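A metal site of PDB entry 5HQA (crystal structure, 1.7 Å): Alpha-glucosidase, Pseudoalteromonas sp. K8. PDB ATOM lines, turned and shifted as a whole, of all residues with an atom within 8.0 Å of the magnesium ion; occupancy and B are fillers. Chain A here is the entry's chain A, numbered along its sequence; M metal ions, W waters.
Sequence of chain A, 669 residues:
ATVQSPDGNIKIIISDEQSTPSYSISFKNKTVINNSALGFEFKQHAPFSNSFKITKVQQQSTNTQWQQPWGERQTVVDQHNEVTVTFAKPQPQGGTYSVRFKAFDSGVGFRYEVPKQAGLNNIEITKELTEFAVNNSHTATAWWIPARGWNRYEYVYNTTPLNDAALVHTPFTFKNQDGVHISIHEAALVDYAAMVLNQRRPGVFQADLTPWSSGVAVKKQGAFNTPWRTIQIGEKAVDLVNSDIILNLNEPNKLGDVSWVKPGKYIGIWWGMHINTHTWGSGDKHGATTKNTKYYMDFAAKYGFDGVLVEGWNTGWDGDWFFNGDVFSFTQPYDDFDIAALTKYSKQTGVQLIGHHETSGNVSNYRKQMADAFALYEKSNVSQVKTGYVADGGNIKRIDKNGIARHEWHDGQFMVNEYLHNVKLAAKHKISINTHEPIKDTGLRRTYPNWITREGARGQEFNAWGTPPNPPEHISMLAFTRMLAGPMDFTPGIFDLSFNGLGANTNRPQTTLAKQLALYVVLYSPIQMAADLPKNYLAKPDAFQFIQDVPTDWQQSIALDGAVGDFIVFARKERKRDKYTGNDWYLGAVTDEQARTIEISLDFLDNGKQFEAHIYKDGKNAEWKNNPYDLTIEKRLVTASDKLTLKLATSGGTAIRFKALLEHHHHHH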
ATOM      1  N   TRP A 143       1.812  17.669  -0.659  1.00  0.00           N
ATOM      2  CA  TRP A 143       1.397  17.185   0.660  1.00  0.00           C
ATOM      3  C   TRP A 143       1.624  15.682   0.677  1.00  0.00           C
ATOM      4  O   TRP A 143       0.907  14.949  -0.015  1.00  0.00           O
ATOM      5  CB  TRP A 143      -0.064  17.525   0.922  1.00  0.00           C
ATOM      6  CG  TRP A 143      -0.408  18.974   0.708  1.00  0.00           C
ATOM      7  CD1 TRP A 143      -0.294  19.981   1.618  1.00  0.00           C
ATOM      8  CD2 TRP A 143      -0.939  19.583  -0.489  1.00  0.00           C
ATOM      9  NE1 TRP A 143      -0.730  21.171   1.074  1.00  0.00           N
ATOM     10  CE2 TRP A 143      -1.126  20.948  -0.217  1.00  0.00           C
ATOM     11  CE3 TRP A 143      -1.291  19.083  -1.750  1.00  0.00           C
ATOM     12  CZ2 TRP A 143      -1.641  21.833  -1.165  1.00  0.00           C
ATOM     13  CZ3 TRP A 143      -1.797  19.966  -2.687  1.00  0.00           C
ATOM     14  CH2 TRP A 143      -1.974  21.321  -2.387  1.00  0.00           C
ATOM     15  N   THR A 159       3.909  19.343   4.341  1.00  0.00           N
ATOM     16  CA  THR A 159       3.540  20.391   3.385  1.00  0.00           C
ATOM     17  C   THR A 159       4.838  21.060   2.952  1.00  0.00           C
ATOM     18  O   THR A 159       5.469  21.770   3.741  1.00  0.00           O
ATOM     19  CB  THR A 159       2.596  21.423   4.008  1.00  0.00           C
ATOM     20  OG1 THR A 159       1.440  20.764   4.544  1.00  0.00           O
ATOM     21  CG2 THR A 159       2.173  22.474   2.966  1.00  0.00           C
ATOM     22  N   PRO A 472      -4.313  18.941  14.199  1.00  0.00           N
ATOM     23  CA  PRO A 472      -5.618  19.397  13.691  1.00  0.00           C
ATOM     24  C   PRO A 472      -5.786  19.262  12.181  1.00  0.00           C
ATOM     25  O   PRO A 472      -6.900  18.967  11.733  1.00  0.00           O
ATOM     26  CB  PRO A 472      -5.652  20.852  14.142  1.00  0.00           C
ATOM     27  CG  PRO A 472      -4.898  20.815  15.443  1.00  0.00           C
ATOM     28  CD  PRO A 472      -3.776  19.850  15.238  1.00  0.00           C
ATOM     29  N   GLU A 473      -4.735  19.454  11.392  1.00  0.00           N
ATOM     30  CA  GLU A 473      -4.871  19.402   9.937  1.00  0.00           C
ATOM     31  C   GLU A 473      -4.977  17.983   9.379  1.00  0.00           C
ATOM     32  O   GLU A 473      -5.184  17.810   8.166  1.00  0.00           O
ATOM     33  CB  GLU A 473      -3.682  20.109   9.270  1.00  0.00           C
ATOM     34  CG  GLU A 473      -2.383  19.325   9.387  1.00  0.00           C
ATOM     35  CD  GLU A 473      -1.198  20.036   8.764  1.00  0.00           C
ATOM     36  OE1 GLU A 473      -1.340  21.188   8.296  1.00  0.00           O
ATOM     37  OE2 GLU A 473      -0.102  19.431   8.768  1.00  0.00           O
ATOM     38  N   HIS A 474      -4.846  16.954  10.220  1.00  0.00           N
ATOM     39  CA  HIS A 474      -4.660  15.591   9.722  1.00  0.00           C
ATOM     40  C   HIS A 474      -5.835  15.138   8.844  1.00  0.00           C
ATOM     41  O   HIS A 474      -5.633  14.578   7.762  1.00  0.00           O
ATOM     42  CB  HIS A 474      -4.456  14.632  10.894  1.00  0.00           C
ATOM     43  CG  HIS A 474      -4.070  13.245  10.476  1.00  0.00           C
ATOM     44  ND1 HIS A 474      -2.966  12.987   9.691  1.00  0.00           N
ATOM     45  CD2 HIS A 474      -4.665  12.046  10.720  1.00  0.00           C
ATOM     46  CE1 HIS A 474      -2.884  11.679   9.472  1.00  0.00           C
ATOM     47  NE2 HIS A 474      -3.905  11.089  10.092  1.00  0.00           N
ATOM     48  N   SER A 476      -8.024  16.870   7.130  1.00  0.00           N
ATOM     49  CA  SER A 476      -8.068  17.582   5.862  1.00  0.00           C
ATOM     50  C   SER A 476      -6.872  17.251   4.975  1.00  0.00           C
ATOM     51  O   SER A 476      -6.890  17.584   3.794  1.00  0.00           O
ATOM     52  CB  SER A 476      -8.154  19.087   6.106  1.00  0.00           C
ATOM     53  OG  SER A 476      -6.962  19.576   6.709  1.00  0.00           O
ATOM     54  N   MET A 477      -5.826  16.617   5.525  1.00  0.00           N
ATOM     55  CA  MET A 477      -4.783  16.014   4.699  1.00  0.00           C
ATOM     56  C   MET A 477      -5.248  14.679   4.137  1.00  0.00           C
ATOM     57  O   MET A 477      -5.170  14.442   2.923  1.00  0.00           O
ATOM     58  CB  MET A 477      -3.497  15.832   5.498  1.00  0.00           C
ATOM     59  CG  MET A 477      -2.818  17.122   5.895  1.00  0.00           C
ATOM     60  SD  MET A 477      -2.139  17.977   4.460  1.00  0.00           S
ATOM     61  CE  MET A 477      -1.284  19.339   5.287  1.00  0.00           C
ATOM     62  N   ALA A 563      -9.964  22.334   0.588  1.00  0.00           N
ATOM     63  CA  ALA A 563      -8.608  22.689   0.203  1.00  0.00           C
ATOM     64  C   ALA A 563      -7.669  21.787   0.990  1.00  0.00           C
ATOM     65  O   ALA A 563      -7.882  21.560   2.177  1.00  0.00           O
ATOM     66  CB  ALA A 563      -8.296  24.170   0.487  1.00  0.00           C
ATOM     67  N   VAL A 564      -6.642  21.264   0.313  1.00  0.00           N
ATOM     68  CA  VAL A 564      -5.803  20.241   0.942  1.00  0.00           C
ATOM     69  C   VAL A 564      -5.167  20.805   2.211  1.00  0.00           C
ATOM     70  O   VAL A 564      -4.549  21.874   2.195  1.00  0.00           O
ATOM     71  CB  VAL A 564      -4.733  19.732  -0.030  1.00  0.00           C
ATOM     72  CG1 VAL A 564      -3.948  18.586   0.635  1.00  0.00           C
ATOM     73  CG2 VAL A 564      -5.358  19.311  -1.350  1.00  0.00           C
ATOM     74  N   GLY A 565      -5.309  20.067   3.314  1.00  0.00           N
ATOM     75  CA  GLY A 565      -4.699  20.492   4.560  1.00  0.00           C
ATOM     76  C   GLY A 565      -5.394  21.651   5.237  1.00  0.00           C
ATOM     77  O   GLY A 565      -4.861  22.173   6.229  1.00  0.00           O
ATOM     78  N   ASP A 566      -6.552  22.076   4.742  1.00  0.00           N
ATOM     79  CA  ASP A 566      -7.329  23.147   5.350  1.00  0.00           C
ATOM     80  C   ASP A 566      -8.735  22.733   5.721  1.00  0.00           C
ATOM     81  O   ASP A 566      -9.130  22.887   6.874  1.00  0.00           O
ATOM     82  CB  ASP A 566      -7.373  24.372   4.416  1.00  0.00           C
ATOM     83  CG  ASP A 566      -6.036  25.077   4.300  1.00  0.00           C
ATOM     84  OD1 ASP A 566      -5.133  24.796   5.129  1.00  0.00           O
ATOM     85  OD2 ASP A 566      -5.897  25.923   3.391  1.00  0.00           O
ATOM     86  N   PHE A 567      -9.524  22.197   4.773  1.00  0.00           N
ATOM     87  CA  PHE A 567     -10.890  21.800   5.119  1.00  0.00           C
ATOM     88  C   PHE A 567     -11.469  20.929   4.019  1.00  0.00           C
ATOM     89  O   PHE A 567     -10.942  20.885   2.901  1.00  0.00           O
ATOM     90  CB  PHE A 567     -11.802  23.011   5.361  1.00  0.00           C
ATOM     91  CG  PHE A 567     -12.197  23.746   4.108  1.00  0.00           C
ATOM     92  CD1 PHE A 567     -11.313  24.622   3.471  1.00  0.00           C
ATOM     93  CD2 PHE A 567     -13.478  23.589   3.561  1.00  0.00           C
ATOM     94  CE1 PHE A 567     -11.689  25.319   2.322  1.00  0.00           C
ATOM     95  CE2 PHE A 567     -13.862  24.272   2.417  1.00  0.00           C
ATOM     96  CZ  PHE A 567     -12.969  25.145   1.790  1.00  0.00           C
ATOM     97  N   THR A 591     -12.334  21.195   9.656  1.00  0.00           N
ATOM     98  CA  THR A 591     -11.289  22.151   9.366  1.00  0.00           C
ATOM     99  C   THR A 591      -9.982  21.679   9.997  1.00  0.00           C
ATOM    100  O   THR A 591      -9.924  20.631  10.656  1.00  0.00           O
ATOM    101  CB  THR A 591     -11.671  23.545   9.852  1.00  0.00           C
ATOM    102  OG1 THR A 591     -10.666  24.494   9.450  1.00  0.00           O
ATOM    103  CG2 THR A 591     -11.820  23.555  11.382  1.00  0.00           C
ATOM    104  N   ASP A 592      -8.936  22.471   9.791  1.00  0.00           N
ATOM    105  CA  ASP A 592      -7.616  22.204  10.353  1.00  0.00           C
ATOM    106  C   ASP A 592      -7.445  22.979  11.656  1.00  0.00           C
ATOM    107  O   ASP A 592      -8.407  23.118  12.427  1.00  0.00           O
ATOM    108  CB  ASP A 592      -6.516  22.570   9.343  1.00  0.00           C
ATOM    109  CG  ASP A 592      -6.608  24.039   8.873  1.00  0.00           C
ATOM    110  OD1 ASP A 592      -7.475  24.774   9.400  1.00  0.00           O
ATOM    111  OD2 ASP A 592      -5.811  24.456   7.997  1.00  0.00           O
ATOM    112  N   GLU A 593      -6.256  23.524  11.925  1.00  0.00           N
ATOM    113  CA  GLU A 593      -6.052  24.250  13.177  1.00  0.00           C
ATOM    114  C   GLU A 593      -6.785  25.592  13.205  1.00  0.00           C
ATOM    115  O   GLU A 593      -6.892  26.194  14.283  1.00  0.00           O
ATOM    116  CB  GLU A 593      -4.554  24.469  13.429  1.00  0.00           C
ATOM    117  CG  GLU A 593      -3.903  25.533  12.529  1.00  0.00           C
ATOM    118  CD  GLU A 593      -3.643  25.046  11.101  1.00  0.00           C
ATOM    119  OE1 GLU A 593      -3.734  23.820  10.836  1.00  0.00           O
ATOM    120  OE2 GLU A 593      -3.356  25.900  10.219  1.00  0.00           O
ATOM    121  N   GLN A 594      -7.300  26.069  12.073  1.00  0.00           N
ATOM    122  CA  GLN A 594      -7.956  27.368  11.999  1.00  0.00           C
ATOM    123  C   GLN A 594      -9.464  27.228  12.069  1.00  0.00           C
ATOM    124  O   GLN A 594     -10.047  26.328  11.452  1.00  0.00           O
ATOM    125  CB  GLN A 594      -7.581  28.092  10.690  1.00  0.00           C
ATOM    126  CG  GLN A 594      -6.115  28.456  10.558  1.00  0.00           C
ATOM    127  CD  GLN A 594      -5.863  29.372   9.366  1.00  0.00           C
ATOM    128  OE1 GLN A 594      -6.811  29.835   8.717  1.00  0.00           O
ATOM    129  NE2 GLN A 594      -4.594  29.646   9.087  1.00  0.00           N
ATOM    130  N   ARG A 596     -12.940  28.278  10.686  1.00  0.00           N
ATOM    131  CA  ARG A 596     -13.275  28.597   9.300  1.00  0.00           C
ATOM    132  C   ARG A 596     -14.773  28.755   9.145  1.00  0.00           C
ATOM    133  O   ARG A 596     -15.551  27.996   9.733  1.00  0.00           O
ATOM    134  CB  ARG A 596     -12.800  27.507   8.313  1.00  0.00           C
ATOM    135  CG  ARG A 596     -11.300  27.464   8.095  1.00  0.00           C
ATOM    136  CD  ARG A 596     -10.827  26.414   7.059  1.00  0.00           C
ATOM    137  NE  ARG A 596      -9.383  26.255   7.245  1.00  0.00           N
ATOM    138  CZ  ARG A 596      -8.475  27.062   6.710  1.00  0.00           C
ATOM    139  NH1 ARG A 596      -8.886  28.041   5.910  1.00  0.00           N
ATOM    140  NH2 ARG A 596      -7.174  26.885   6.952  1.00  0.00           N
HETATM  141 MG    MG M   1      -4.172  24.002   6.788  1.00  0.00          MG
HETATM  142  O   HOH W   1      -3.039  23.229   8.285  1.00  0.00           O
HETATM  143  O   HOH W   2      -3.506  25.886   7.389  1.00  0.00           O
HETATM  144  O   HOH W   3      -2.518  23.783   5.543  1.00  0.00           O
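The nearest printed residue that does not touch the magnesium ion is Glu 593 (4.005 Å).
The backbone NH (N) of Gly 565 is in hydrogen-bond range of the backbone carbonyl oxygen (O) of Ser 476, 3.0 Å away.
The side-chain carboxylate (OD2) of Asp 566 is in salt-bridge range of the guanidinium group (NH2) of Arg 596 (3.9 Å).
OG of Ser 476 sits at hydrogen-bond distance from N of Asp 566, at 3.2 Å.
The side-chain hydroxyl (OG1) of Thr 591 lies close to the backbone carbonyl oxygen (O) of Asp 566 (3.4 Å).
The guanidinium group (NE) of Arg 596 lies within salt-bridge range of the side-chain carboxylate (OD1) of Asp 592 (3.2 Å).
The side-chain carboxylate of Asp 592 sits at hydrogen-bond distance from the backbone NH of Gln 594 (3.0 Å).
The side-chain carboxylate of Asp 592 sits at hydrogen-bond distance from the side-chain hydroxyl of Thr 591, at 3.2 Å.
Water W1 bridges OE1 of Glu 473 (2.7 Å) and OE1 of Glu 593 (2.7 Å).
Water W1 binds the magnesium ion (2.0 Å).
The magnesium ion is bound by the backbone carbonyl oxygen (O) of Gly 565, at 2.0 Å.
The magnesium ion is bound by the side-chain carboxylate (OD1) of Asp 566 (2.1 Å).
Water W3 is bound to the magnesium ion.
Water W2 binds the magnesium ion (2.1 Å).
The side-chain carboxylate (OD2) of Asp 592 binds the magnesium ion (2.1 Å).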
